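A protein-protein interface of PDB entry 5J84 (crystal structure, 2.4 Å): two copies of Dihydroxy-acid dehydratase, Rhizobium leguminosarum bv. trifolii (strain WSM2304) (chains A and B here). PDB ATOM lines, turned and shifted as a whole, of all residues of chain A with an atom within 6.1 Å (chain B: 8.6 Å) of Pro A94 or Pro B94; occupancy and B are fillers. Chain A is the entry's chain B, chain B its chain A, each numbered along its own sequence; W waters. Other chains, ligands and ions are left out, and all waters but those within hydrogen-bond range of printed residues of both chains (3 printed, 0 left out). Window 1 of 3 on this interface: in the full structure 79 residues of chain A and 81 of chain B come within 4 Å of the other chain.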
ATOM      1  N   ILE A  58     -16.553 -26.425 -14.061  1.00  0.00           N
ATOM      2  CA  ILE A  58     -17.725 -26.648 -14.895  1.00  0.00           C
ATOM      3  C   ILE A  58     -18.098 -25.344 -15.599  1.00  0.00           C
ATOM      4  O   ILE A  58     -18.761 -24.480 -15.027  1.00  0.00           O
ATOM      5  CB  ILE A  58     -18.905 -27.177 -14.064  1.00  0.00           C
ATOM      6  CG1 ILE A  58     -18.486 -28.445 -13.315  1.00  0.00           C
ATOM      7  CG2 ILE A  58     -20.118 -27.430 -14.948  1.00  0.00           C
ATOM      8  CD1 ILE A  58     -19.408 -28.825 -12.180  1.00  0.00           C
ATOM      9  N   LEU A  59     -17.660 -25.212 -16.846  1.00  0.00           N
ATOM     10  CA  LEU A  59     -17.810 -23.969 -17.595  1.00  0.00           C
ATOM     11  C   LEU A  59     -19.195 -23.868 -18.214  1.00  0.00           C
ATOM     12  O   LEU A  59     -19.523 -24.593 -19.153  1.00  0.00           O
ATOM     13  CB  LEU A  59     -16.738 -23.839 -18.683  1.00  0.00           C
ATOM     14  CG  LEU A  59     -15.241 -23.841 -18.334  1.00  0.00           C
ATOM     15  CD1 LEU A  59     -14.742 -25.189 -17.851  1.00  0.00           C
ATOM     16  CD2 LEU A  59     -14.424 -23.378 -19.528  1.00  0.00           C
ATOM     17  N   ASN A  60     -20.000 -22.960 -17.676  1.00  0.00           N
ATOM     18  CA  ASN A  60     -21.399 -22.855 -18.056  1.00  0.00           C
ATOM     19  C   ASN A  60     -21.694 -21.655 -18.955  1.00  0.00           C
ATOM     20  O   ASN A  60     -21.398 -20.512 -18.608  1.00  0.00           O
ATOM     21  CB  ASN A  60     -22.263 -22.789 -16.799  1.00  0.00           C
ATOM     22  CG  ASN A  60     -23.686 -23.206 -17.055  1.00  0.00           C
ATOM     23  OD1 ASN A  60     -24.142 -23.226 -18.197  1.00  0.00           O
ATOM     24  ND2 ASN A  60     -24.397 -23.551 -15.991  1.00  0.00           N
ATOM     25  N   THR A  61     -22.293 -21.930 -20.108  1.00  0.00           N
ATOM     26  CA  THR A  61     -22.681 -20.886 -21.047  1.00  0.00           C
ATOM     27  C   THR A  61     -24.152 -20.522 -20.897  1.00  0.00           C
ATOM     28  O   THR A  61     -24.741 -19.915 -21.789  1.00  0.00           O
ATOM     29  CB  THR A  61     -22.417 -21.305 -22.502  1.00  0.00           C
ATOM     30  OG1 THR A  61     -23.064 -22.555 -22.757  1.00  0.00           O
ATOM     31  CG2 THR A  61     -20.930 -21.461 -22.747  1.00  0.00           C
ATOM     32  N   TRP A  62     -24.747 -20.910 -19.774  1.00  0.00           N
ATOM     33  CA  TRP A  62     -26.113 -20.507 -19.476  1.00  0.00           C
ATOM     34  C   TRP A  62     -26.207 -18.989 -19.403  1.00  0.00           C
ATOM     35  O   TRP A  62     -25.282 -18.319 -18.951  1.00  0.00           O
ATOM     36  CB  TRP A  62     -26.607 -21.121 -18.161  1.00  0.00           C
ATOM     37  CG  TRP A  62     -27.926 -20.549 -17.730  1.00  0.00           C
ATOM     38  CD1 TRP A  62     -29.163 -21.001 -18.074  1.00  0.00           C
ATOM     39  CD2 TRP A  62     -28.136 -19.396 -16.900  1.00  0.00           C
ATOM     40  NE1 TRP A  62     -30.132 -20.208 -17.506  1.00  0.00           N
ATOM     41  CE2 TRP A  62     -29.527 -19.216 -16.781  1.00  0.00           C
ATOM     42  CE3 TRP A  62     -27.281 -18.500 -16.248  1.00  0.00           C
ATOM     43  CZ2 TRP A  62     -30.084 -18.179 -16.034  1.00  0.00           C
ATOM     44  CZ3 TRP A  62     -27.836 -17.475 -15.505  1.00  0.00           C
ATOM     45  CH2 TRP A  62     -29.225 -17.324 -15.401  1.00  0.00           C
ATOM     46  N   SER A  63     -27.339 -18.463 -19.845  1.00  0.00           N
ATOM     47  CA  SER A  63     -27.646 -17.048 -19.722  1.00  0.00           C
ATOM     48  C   SER A  63     -29.124 -16.847 -19.989  1.00  0.00           C
ATOM     49  O   SER A  63     -29.732 -17.620 -20.728  1.00  0.00           O
ATOM     50  CB  SER A  63     -26.815 -16.216 -20.694  1.00  0.00           C
ATOM     51  OG  SER A  63     -27.343 -14.907 -20.805  1.00  0.00           O
ATOM     52  N   ASP A  64     -29.713 -15.828 -19.374  1.00  0.00           N
ATOM     53  CA  ASP A  64     -31.111 -15.527 -19.643  1.00  0.00           C
ATOM     54  C   ASP A  64     -31.260 -14.988 -21.063  1.00  0.00           C
ATOM     55  O   ASP A  64     -32.342 -15.057 -21.646  1.00  0.00           O
ATOM     56  CB  ASP A  64     -31.667 -14.529 -18.628  1.00  0.00           C
ATOM     57  CG  ASP A  64     -32.182 -15.200 -17.366  1.00  0.00           C
ATOM     58  OD1 ASP A  64     -32.535 -16.398 -17.420  1.00  0.00           O
ATOM     59  OD2 ASP A  64     -32.252 -14.521 -16.321  1.00  0.00           O
ATOM     60  N   GLU A  92     -18.570 -24.426 -10.435  1.00  0.00           N
ATOM     61  CA  GLU A  92     -19.214 -23.870 -11.613  1.00  0.00           C
ATOM     62  C   GLU A  92     -18.651 -22.497 -11.944  1.00  0.00           C
ATOM     63  O   GLU A  92     -18.589 -21.612 -11.090  1.00  0.00           O
ATOM     64  CB  GLU A  92     -20.724 -23.777 -11.410  1.00  0.00           C
ATOM     65  CG  GLU A  92     -21.474 -23.266 -12.626  1.00  0.00           C
ATOM     66  CD  GLU A  92     -22.974 -23.230 -12.419  1.00  0.00           C
ATOM     67  OE1 GLU A  92     -23.682 -22.745 -13.325  1.00  0.00           O
ATOM     68  OE2 GLU A  92     -23.444 -23.679 -11.353  1.00  0.00           O
ATOM     69  N   VAL A  93     -18.248 -22.324 -13.195  1.00  0.00           N
ATOM     70  CA  VAL A  93     -17.674 -21.068 -13.647  1.00  0.00           C
ATOM     71  C   VAL A  93     -18.372 -20.609 -14.918  1.00  0.00           C
ATOM     72  O   VAL A  93     -18.151 -21.172 -15.988  1.00  0.00           O
ATOM     73  CB  VAL A  93     -16.168 -21.188 -13.912  1.00  0.00           C
ATOM     74  CG1 VAL A  93     -15.597 -19.840 -14.322  1.00  0.00           C
ATOM     75  CG2 VAL A  93     -15.460 -21.712 -12.683  1.00  0.00           C
ATOM     76  N   PRO A  94     -19.247 -19.605 -14.798  1.00  0.00           N
ATOM     77  CA  PRO A  94     -19.908 -19.011 -15.964  1.00  0.00           C
ATOM     78  C   PRO A  94     -18.906 -18.414 -16.955  1.00  0.00           C
ATOM     79  O   PRO A  94     -17.957 -17.741 -16.540  1.00  0.00           O
ATOM     80  CB  PRO A  94     -20.781 -17.916 -15.351  1.00  0.00           C
ATOM     81  CG  PRO A  94     -21.011 -18.356 -13.943  1.00  0.00           C
ATOM     82  CD  PRO A  94     -19.745 -19.042 -13.532  1.00  0.00           C
ATOM     83  N   VAL A  95     -19.104 -18.674 -18.245  1.00  0.00           N
ATOM     84  CA  VAL A  95     -18.240 -18.110 -19.278  1.00  0.00           C
ATOM     85  C   VAL A  95     -19.077 -17.410 -20.339  1.00  0.00           C
ATOM     86  O   VAL A  95     -20.284 -17.635 -20.427  1.00  0.00           O
ATOM     87  CB  VAL A  95     -17.357 -19.187 -19.942  1.00  0.00           C
ATOM     88  CG1 VAL A  95     -16.389 -19.777 -18.928  1.00  0.00           C
ATOM     89  CG2 VAL A  95     -18.210 -20.280 -20.553  1.00  0.00           C
ATOM     90  N   PHE A  96     -18.425 -16.559 -21.127  1.00  0.00           N
ATOM     91  CA  PHE A  96     -19.078 -15.771 -22.174  1.00  0.00           C
ATOM     92  C   PHE A  96     -19.959 -16.635 -23.069  1.00  0.00           C
ATOM     93  O   PHE A  96     -19.528 -17.676 -23.561  1.00  0.00           O
ATOM     94  CB  PHE A  96     -18.027 -15.043 -23.022  1.00  0.00           C
ATOM     95  CG  PHE A  96     -18.578 -13.896 -23.834  1.00  0.00           C
ATOM     96  CD1 PHE A  96     -19.222 -14.121 -25.040  1.00  0.00           C
ATOM     97  CD2 PHE A  96     -18.419 -12.590 -23.404  1.00  0.00           C
ATOM     98  CE1 PHE A  96     -19.717 -13.065 -25.785  1.00  0.00           C
ATOM     99  CE2 PHE A  96     -18.909 -11.532 -24.147  1.00  0.00           C
ATOM    100  CZ  PHE A  96     -19.558 -11.770 -25.338  1.00  0.00           C
ATOM    101  N   SER A  97     -21.195 -16.199 -23.279  1.00  0.00           N
ATOM    102  CA  SER A  97     -22.149 -16.986 -24.050  1.00  0.00           C
ATOM    103  C   SER A  97     -22.643 -16.232 -25.276  1.00  0.00           C
ATOM    104  O   SER A  97     -23.525 -15.382 -25.178  1.00  0.00           O
ATOM    105  CB  SER A  97     -23.336 -17.390 -23.177  1.00  0.00           C
ATOM    106  OG  SER A  97     -24.277 -18.137 -23.922  1.00  0.00           O
ATOM    107  N   GLY B  57     -30.770  -5.937 -18.178  1.00  0.00           N
ATOM    108  CA  GLY B  57     -29.711  -6.923 -18.125  1.00  0.00           C
ATOM    109  C   GLY B  57     -29.083  -6.923 -16.745  1.00  0.00           C
ATOM    110  O   GLY B  57     -28.509  -5.924 -16.316  1.00  0.00           O
ATOM    111  N   ILE B  58     -29.206  -8.040 -16.041  1.00  0.00           N
ATOM    112  CA  ILE B  58     -28.632  -8.150 -14.709  1.00  0.00           C
ATOM    113  C   ILE B  58     -27.262  -8.812 -14.827  1.00  0.00           C
ATOM    114  O   ILE B  58     -27.155 -10.032 -14.936  1.00  0.00           O
ATOM    115  CB  ILE B  58     -29.553  -8.942 -13.768  1.00  0.00           C
ATOM    116  CG1 ILE B  58     -30.921  -8.263 -13.691  1.00  0.00           C
ATOM    117  CG2 ILE B  58     -28.937  -9.053 -12.384  1.00  0.00           C
ATOM    118  CD1 ILE B  58     -32.009  -9.130 -13.136  1.00  0.00           C
ATOM    119  N   LEU B  59     -26.220  -7.987 -14.820  1.00  0.00           N
ATOM    120  CA  LEU B  59     -24.869  -8.458 -15.091  1.00  0.00           C
ATOM    121  C   LEU B  59     -24.237  -9.047 -13.841  1.00  0.00           C
ATOM    122  O   LEU B  59     -23.829  -8.320 -12.939  1.00  0.00           O
ATOM    123  CB  LEU B  59     -24.018  -7.309 -15.621  1.00  0.00           C
ATOM    124  CG  LEU B  59     -24.578  -6.611 -16.861  1.00  0.00           C
ATOM    125  CD1 LEU B  59     -23.548  -5.657 -17.442  1.00  0.00           C
ATOM    126  CD2 LEU B  59     -25.057  -7.611 -17.905  1.00  0.00           C
ATOM    127  N   ASN B  60     -24.126 -10.368 -13.808  1.00  0.00           N
ATOM    128  CA  ASN B  60     -23.697 -11.053 -12.599  1.00  0.00           C
ATOM    129  C   ASN B  60     -22.269 -11.577 -12.688  1.00  0.00           C
ATOM    130  O   ASN B  60     -21.925 -12.322 -13.606  1.00  0.00           O
ATOM    131  CB  ASN B  60     -24.650 -12.205 -12.286  1.00  0.00           C
ATOM    132  CG  ASN B  60     -24.609 -12.608 -10.835  1.00  0.00           C
ATOM    133  OD1 ASN B  60     -23.669 -12.274 -10.118  1.00  0.00           O
ATOM    134  ND2 ASN B  60     -25.621 -13.344 -10.394  1.00  0.00           N
ATOM    135  N   THR B  61     -21.444 -11.186 -11.722  1.00  0.00           N
ATOM    136  CA  THR B  61     -20.064 -11.648 -11.654  1.00  0.00           C
ATOM    137  C   THR B  61     -19.927 -12.812 -10.683  1.00  0.00           C
ATOM    138  O   THR B  61     -18.827 -13.140 -10.252  1.00  0.00           O
ATOM    139  CB  THR B  61     -19.105 -10.531 -11.217  1.00  0.00           C
ATOM    140  OG1 THR B  61     -19.534  -9.998  -9.960  1.00  0.00           O
ATOM    141  CG2 THR B  61     -19.070  -9.423 -12.252  1.00  0.00           C
ATOM    142  N   TRP B  62     -21.052 -13.432 -10.343  1.00  0.00           N
ATOM    143  CA  TRP B  62     -21.030 -14.617  -9.501  1.00  0.00           C
ATOM    144  C   TRP B  62     -20.204 -15.705 -10.162  1.00  0.00           C
ATOM    145  O   TRP B  62     -20.186 -15.826 -11.386  1.00  0.00           O
ATOM    146  CB  TRP B  62     -22.446 -15.142  -9.236  1.00  0.00           C
ATOM    147  CG  TRP B  62     -22.437 -16.479  -8.549  1.00  0.00           C
ATOM    148  CD1 TRP B  62     -22.436 -16.710  -7.209  1.00  0.00           C
ATOM    149  CD2 TRP B  62     -22.369 -17.768  -9.177  1.00  0.00           C
ATOM    150  NE1 TRP B  62     -22.398 -18.060  -6.960  1.00  0.00           N
ATOM    151  CE2 TRP B  62     -22.350 -18.730  -8.153  1.00  0.00           C
ATOM    152  CE3 TRP B  62     -22.326 -18.198 -10.508  1.00  0.00           C
ATOM    153  CZ2 TRP B  62     -22.289 -20.095  -8.415  1.00  0.00           C
ATOM    154  CZ3 TRP B  62     -22.268 -19.552 -10.765  1.00  0.00           C
ATOM    155  CH2 TRP B  62     -22.253 -20.485  -9.726  1.00  0.00           C
ATOM    156  N   SER B  63     -19.513 -16.484  -9.338  1.00  0.00           N
ATOM    157  CA  SER B  63     -18.794 -17.667  -9.785  1.00  0.00           C
ATOM    158  C   SER B  63     -18.401 -18.496  -8.568  1.00  0.00           C
ATOM    159  O   SER B  63     -18.183 -17.951  -7.488  1.00  0.00           O
ATOM    160  CB  SER B  63     -17.555 -17.283 -10.598  1.00  0.00           C
ATOM    161  OG  SER B  63     -16.688 -18.392 -10.753  1.00  0.00           O
ATOM    162  N   ASP B  64     -18.313 -19.812  -8.736  1.00  0.00           N
ATOM    163  CA  ASP B  64     -17.874 -20.666  -7.640  1.00  0.00           C
ATOM    164  C   ASP B  64     -16.398 -20.424  -7.350  1.00  0.00           C
ATOM    165  O   ASP B  64     -15.914 -20.735  -6.261  1.00  0.00           O
ATOM    166  CB  ASP B  64     -18.132 -22.141  -7.945  1.00  0.00           C
ATOM    167  CG  ASP B  64     -19.531 -22.579  -7.545  1.00  0.00           C
ATOM    168  OD1 ASP B  64     -20.120 -21.927  -6.659  1.00  0.00           O
ATOM    169  OD2 ASP B  64     -20.036 -23.578  -8.101  1.00  0.00           O
ATOM    170  N   MET B  65     -15.691 -19.862  -8.327  1.00  0.00           N
ATOM    171  CA  MET B  65     -14.290 -19.505  -8.152  1.00  0.00           C
ATOM    172  C   MET B  65     -14.118 -18.037  -7.786  1.00  0.00           C
ATOM    173  O   MET B  65     -13.016 -17.502  -7.849  1.00  0.00           O
ATOM    174  CB  MET B  65     -13.492 -19.824  -9.412  1.00  0.00           C
ATOM    175  CG  MET B  65     -13.462 -21.297  -9.745  1.00  0.00           C
ATOM    176  SD  MET B  65     -11.829 -21.825 -10.272  1.00  0.00           S
ATOM    177  CE  MET B  65     -12.123 -23.557 -10.616  1.00  0.00           C
ATOM    178  N   THR B  66     -15.214 -17.387  -7.411  1.00  0.00           N
ATOM    179  CA  THR B  66     -15.152 -16.031  -6.870  1.00  0.00           C
ATOM    180  C   THR B  66     -15.941 -16.002  -5.565  1.00  0.00           C
ATOM    181  O   THR B  66     -17.037 -15.444  -5.505  1.00  0.00           O
ATOM    182  CB  THR B  66     -15.700 -14.984  -7.861  1.00  0.00           C
ATOM    183  OG1 THR B  66     -15.020 -15.116  -9.114  1.00  0.00           O
ATOM    184  CG2 THR B  66     -15.477 -13.572  -7.336  1.00  0.00           C
ATOM    185  N   ARG B  73     -25.983 -14.866  -6.778  1.00  0.00           N
ATOM    186  CA  ARG B  73     -27.138 -15.405  -7.493  1.00  0.00           C
ATOM    187  C   ARG B  73     -28.417 -15.121  -6.717  1.00  0.00           C
ATOM    188  O   ARG B  73     -29.460 -14.842  -7.305  1.00  0.00           O
ATOM    189  CB  ARG B  73     -26.999 -16.906  -7.760  1.00  0.00           C
ATOM    190  CG  ARG B  73     -26.029 -17.234  -8.882  1.00  0.00           C
ATOM    191  CD  ARG B  73     -25.953 -18.728  -9.153  1.00  0.00           C
ATOM    192  NE  ARG B  73     -25.594 -19.505  -7.972  1.00  0.00           N
ATOM    193  CZ  ARG B  73     -25.411 -20.820  -7.981  1.00  0.00           C
ATOM    194  NH1 ARG B  73     -25.536 -21.496  -9.117  1.00  0.00           N
ATOM    195  NH2 ARG B  73     -25.086 -21.459  -6.866  1.00  0.00           N
ATOM    196  N   LEU B  91     -33.372  -9.999 -17.005  1.00  0.00           N
ATOM    197  CA  LEU B  91     -32.626 -11.116 -17.565  1.00  0.00           C
ATOM    198  C   LEU B  91     -31.236 -11.194 -16.945  1.00  0.00           C
ATOM    199  O   LEU B  91     -30.445 -10.257 -17.059  1.00  0.00           O
ATOM    200  CB  LEU B  91     -32.514 -10.982 -19.084  1.00  0.00           C
ATOM    201  CG  LEU B  91     -33.811 -10.995 -19.894  1.00  0.00           C
ATOM    202  CD1 LEU B  91     -33.543 -10.505 -21.304  1.00  0.00           C
ATOM    203  CD2 LEU B  91     -34.433 -12.383 -19.919  1.00  0.00           C
ATOM    204  N   GLU B  92     -30.944 -12.307 -16.279  1.00  0.00           N
ATOM    205  CA  GLU B  92     -29.651 -12.471 -15.635  1.00  0.00           C
ATOM    206  C   GLU B  92     -28.614 -12.882 -16.672  1.00  0.00           C
ATOM    207  O   GLU B  92     -28.807 -13.842 -17.416  1.00  0.00           O
ATOM    208  CB  GLU B  92     -29.728 -13.501 -14.508  1.00  0.00           C
ATOM    209  CG  GLU B  92     -28.427 -13.659 -13.730  1.00  0.00           C
ATOM    210  CD  GLU B  92     -28.548 -14.634 -12.572  1.00  0.00           C
ATOM    211  OE1 GLU B  92     -27.530 -14.873 -11.888  1.00  0.00           O
ATOM    212  OE2 GLU B  92     -29.663 -15.143 -12.329  1.00  0.00           O
ATOM    213  N   VAL B  93     -27.505 -12.158 -16.705  1.00  0.00           N
ATOM    214  CA  VAL B  93     -26.458 -12.416 -17.679  1.00  0.00           C
ATOM    215  C   VAL B  93     -25.116 -12.551 -16.980  1.00  0.00           C
ATOM    216  O   VAL B  93     -24.528 -11.556 -16.561  1.00  0.00           O
ATOM    217  CB  VAL B  93     -26.369 -11.291 -18.728  1.00  0.00           C
ATOM    218  CG1 VAL B  93     -25.294 -11.609 -19.755  1.00  0.00           C
ATOM    219  CG2 VAL B  93     -27.713 -11.080 -19.399  1.00  0.00           C
ATOM    220  N   PRO B  94     -24.638 -13.791 -16.831  1.00  0.00           N
ATOM    221  CA  PRO B  94     -23.311 -14.011 -16.253  1.00  0.00           C
ATOM    222  C   PRO B  94     -22.228 -13.343 -17.089  1.00  0.00           C
ATOM    223  O   PRO B  94     -22.222 -13.484 -18.311  1.00  0.00           O
ATOM    224  CB  PRO B  94     -23.167 -15.532 -16.280  1.00  0.00           C
ATOM    225  CG  PRO B  94     -24.572 -16.044 -16.276  1.00  0.00           C
ATOM    226  CD  PRO B  94     -25.356 -15.054 -17.075  1.00  0.00           C
ATOM    227  N   VAL B  95     -21.324 -12.627 -16.431  1.00  0.00           N
ATOM    228  CA  VAL B  95     -20.225 -11.968 -17.120  1.00  0.00           C
ATOM    229  C   VAL B  95     -18.894 -12.330 -16.471  1.00  0.00           C
ATOM    230  O   VAL B  95     -18.864 -12.817 -15.339  1.00  0.00           O
ATOM    231  CB  VAL B  95     -20.398 -10.436 -17.126  1.00  0.00           C
ATOM    232  CG1 VAL B  95     -21.634 -10.050 -17.921  1.00  0.00           C
ATOM    233  CG2 VAL B  95     -20.492  -9.913 -15.712  1.00  0.00           C
ATOM    234  N   PHE B  96     -17.804 -12.096 -17.199  1.00  0.00           N
ATOM    235  CA  PHE B  96     -16.460 -12.412 -16.724  1.00  0.00           C
ATOM    236  C   PHE B  96     -16.218 -11.883 -15.322  1.00  0.00           C
ATOM    237  O   PHE B  96     -16.475 -10.715 -15.030  1.00  0.00           O
ATOM    238  CB  PHE B  96     -15.402 -11.851 -17.678  1.00  0.00           C
ATOM    239  CG  PHE B  96     -14.032 -12.443 -17.479  1.00  0.00           C
ATOM    240  CD1 PHE B  96     -13.190 -11.961 -16.491  1.00  0.00           C
ATOM    241  CD2 PHE B  96     -13.593 -13.488 -18.273  1.00  0.00           C
ATOM    242  CE1 PHE B  96     -11.934 -12.506 -16.305  1.00  0.00           C
ATOM    243  CE2 PHE B  96     -12.339 -14.036 -18.092  1.00  0.00           C
ATOM    244  CZ  PHE B  96     -11.509 -13.543 -17.105  1.00  0.00           C
ATOM    245  N   SER B  97     -15.720 -12.756 -14.458  1.00  0.00           N
ATOM    246  CA  SER B  97     -15.510 -12.414 -13.060  1.00  0.00           C
ATOM    247  C   SER B  97     -14.038 -12.570 -12.701  1.00  0.00           C
ATOM    248  O   SER B  97     -13.554 -13.682 -12.489  1.00  0.00           O
ATOM    249  CB  SER B  97     -16.384 -13.291 -12.161  1.00  0.00           C
ATOM    250  OG  SER B  97     -16.196 -12.979 -10.792  1.00  0.00           O
ATOM    251  N   PHE B 103      -7.191 -15.903  -9.708  1.00  0.00           N
ATOM    252  CA  PHE B 103      -6.454 -15.627 -10.939  1.00  0.00           C
ATOM    253  C   PHE B 103      -4.964 -15.396 -10.729  1.00  0.00           C
ATOM    254  O   PHE B 103      -4.552 -14.632  -9.857  1.00  0.00           O
ATOM    255  CB  PHE B 103      -7.052 -14.421 -11.664  1.00  0.00           C
ATOM    256  CG  PHE B 103      -8.055 -14.791 -12.719  1.00  0.00           C
ATOM    257  CD1 PHE B 103      -7.640 -15.333 -13.925  1.00  0.00           C
ATOM    258  CD2 PHE B 103      -9.408 -14.579 -12.515  1.00  0.00           C
ATOM    259  CE1 PHE B 103      -8.553 -15.671 -14.901  1.00  0.00           C
ATOM    260  CE2 PHE B 103     -10.328 -14.914 -13.489  1.00  0.00           C
ATOM    261  CZ  PHE B 103      -9.899 -15.462 -14.684  1.00  0.00           C
ATOM    262  N   ALA B 117     -15.459  -7.771 -22.501  1.00  0.00           N
ATOM    263  CA  ALA B 117     -16.572  -8.698 -22.658  1.00  0.00           C
ATOM    264  C   ALA B 117     -17.881  -8.087 -22.159  1.00  0.00           C
ATOM    265  O   ALA B 117     -18.940  -8.302 -22.749  1.00  0.00           O
ATOM    266  CB  ALA B 117     -16.281  -9.999 -21.931  1.00  0.00           C
ATOM    267  N   VAL B 118     -17.806  -7.340 -21.062  1.00  0.00           N
ATOM    268  CA  VAL B 118     -18.983  -6.668 -20.517  1.00  0.00           C
ATOM    269  C   VAL B 118     -19.537  -5.667 -21.525  1.00  0.00           C
ATOM    270  O   VAL B 118     -20.743  -5.618 -21.765  1.00  0.00           O
ATOM    271  CB  VAL B 118     -18.663  -5.946 -19.188  1.00  0.00           C
ATOM    272  CG1 VAL B 118     -19.760  -4.959 -18.828  1.00  0.00           C
ATOM    273  CG2 VAL B 118     -18.473  -6.956 -18.074  1.00  0.00           C
ATOM    274  N   ALA B 121     -21.194  -7.576 -24.337  1.00  0.00           N
ATOM    275  CA  ALA B 121     -22.402  -8.240 -23.877  1.00  0.00           C
ATOM    276  C   ALA B 121     -23.550  -7.240 -23.758  1.00  0.00           C
ATOM    277  O   ALA B 121     -24.708  -7.574 -24.010  1.00  0.00           O
ATOM    278  CB  ALA B 121     -22.154  -8.928 -22.545  1.00  0.00           C
ATOM    279  N   GLN B 125     -26.423  -7.087 -27.200  1.00  0.00           N
ATOM    280  CA  GLN B 125     -27.616  -7.836 -26.824  1.00  0.00           C
ATOM    281  C   GLN B 125     -28.774  -6.904 -26.454  1.00  0.00           C
ATOM    282  O   GLN B 125     -28.547  -5.746 -26.108  1.00  0.00           O
ATOM    283  CB  GLN B 125     -27.284  -8.785 -25.671  1.00  0.00           C
ATOM    284  CG  GLN B 125     -26.300  -9.873 -26.061  1.00  0.00           C
ATOM    285  CD  GLN B 125     -26.121 -10.907 -24.977  1.00  0.00           C
ATOM    286  OE1 GLN B 125     -26.533 -12.056 -25.131  1.00  0.00           O
ATOM    287  NE2 GLN B 125     -25.514 -10.505 -23.868  1.00  0.00           N
ATOM    288  N   LEU B 133     -23.906  -6.432 -10.866  1.00  0.00           N
ATOM    289  CA  LEU B 133     -23.661  -7.223  -9.661  1.00  0.00           C
ATOM    290  C   LEU B 133     -22.179  -7.529  -9.489  1.00  0.00           C
ATOM    291  O   LEU B 133     -21.622  -8.354 -10.211  1.00  0.00           O
ATOM    292  CB  LEU B 133     -24.452  -8.532  -9.691  1.00  0.00           C
ATOM    293  CG  LEU B 133     -25.940  -8.490  -9.347  1.00  0.00           C
ATOM    294  CD1 LEU B 133     -26.574  -9.840  -9.606  1.00  0.00           C
ATOM    295  CD2 LEU B 133     -26.126  -8.102  -7.898  1.00  0.00           C
ATOM    296  N   LEU B 143     -16.676  -3.773 -14.545  1.00  0.00           N
ATOM    297  CA  LEU B 143     -18.041  -3.611 -15.020  1.00  0.00           C
ATOM    298  C   LEU B 143     -18.365  -2.129 -15.179  1.00  0.00           C
ATOM    299  O   LEU B 143     -19.147  -1.751 -16.047  1.00  0.00           O
ATOM    300  CB  LEU B 143     -19.032  -4.298 -14.081  1.00  0.00           C
ATOM    301  CG  LEU B 143     -19.407  -5.710 -14.544  1.00  0.00           C
ATOM    302  CD1 LEU B 143     -18.218  -6.653 -14.427  1.00  0.00           C
ATOM    303  CD2 LEU B 143     -20.602  -6.249 -13.777  1.00  0.00           C
HETATM  304  O   HOH W   1     -23.894 -24.058  -8.469  1.00  0.00           O
HETATM  305  O   HOH W   2     -25.692 -13.614 -23.291  1.00  0.00           O
HETATM  306  O   HOH W   3     -17.580 -15.495 -17.494  1.00  0.00           O
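N of Glu A92 sits at hydrogen-bond distance from OD2 of Asp B64, at 2.9 Å.
The side-chain carboxylate (OE2) of Glu A92 is in salt-bridge range of the guanidinium group (NH1) of Arg B73 (3.8 Å).
The side-chain carboxylate of Asp A64 is in hydrogen-bond range of the backbone NH of Glu B92.
Water W3 bridges O of Pro A94 (2.5 Å) and N of Phe B96 (3.4 Å).
Water W2 lies within hydrogen-bond range of the side-chain amide oxygen (OE1) of Gln B125 (2.6 Å), the side-chain hydroxyl (OG) of Ser A63 (3.3 Å) and the backbone carbonyl oxygen (O) of Ser A97 (3.4 Å).
Water W1 lies within hydrogen-bond range of OE2 of Glu A92 and NH1 of Arg B73.
Hydrophobic or aromatic side chains of chain B that line the printed part of chain A: Trp B62, Met B65, Leu B91, Pro B94 and Ala B117.
Hydrophobic or aromatic side chains of chain A that line the printed part of chain B: Trp A62, Val A93, Pro A94 and Phe A96.
Trp A62 touches Glu B92, and with the chains exchanged Glu A92 touches Trp B62.
Trp A62 touches Pro B94, and with the chains exchanged Pro A94 touches Trp B62.
Ser A63 touches Glu B92, and with the chains exchanged Glu A92 touches Ser B63.
Asp A64 touches Glu B92, and with the chains exchanged Glu A92 touches Asp B64.
Positions printed for both chains: 58, 59, 60, 61, 62, 63, 64, 92, 93, 94, 95, 96 and 97.
Of the 13 pairs that touch across the chains among the printed residues, 9 have their exchanged pair printed and touching as well.
N of Ile B58 is in hydrogen-bond range of O of Leu B91.
OD1 of Asn B60 lies within hydrogen-bond range of N of Trp B62 (2.9 Å).
The side-chain hydroxyl of Ser B63 is in hydrogen-bond range of the backbone NH of Met B65 (3.0 Å).
The backbone carbonyl oxygen (O) of Ile A58 lies within hydrogen-bond range of the backbone NH (N) of Val A93 (2.9 Å).
The side-chain amide oxygen of Asn A60 is in hydrogen-bond range of the backbone NH of Trp A62 (2.9 Å).
ND2 of Asn A60 lies within hydrogen-bond range of OE1 of Glu A92 (2.9 Å).
Of the printed residues of chain B, Ser A63 touches Glu B92 (3.8 Å).
Leu B59 touches none of the printed residues of chain A.
Of the printed residues of chain A, Ser B63 touches Glu A92.
Of chain A, only Trp A62 and Pro A94 come within 4 Å of Pro B94.
The nearest residue of chain A that does not touch Pro B94 is Ser A63 (4.03 Å).
Among the printed residues, pairs that only touch across the chains: Trp A62 with Glu B92, Trp A62 with Pro B94, Ser A63 with Glu B92, Asp A64 with Leu B91, Glu A92 with Trp B62, Glu A92 with Ser B63, Val A93 with Met B65, Pro A94 with Trp B62, Pro A94 with Pro B94 and Phe A96 with Ala B117.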
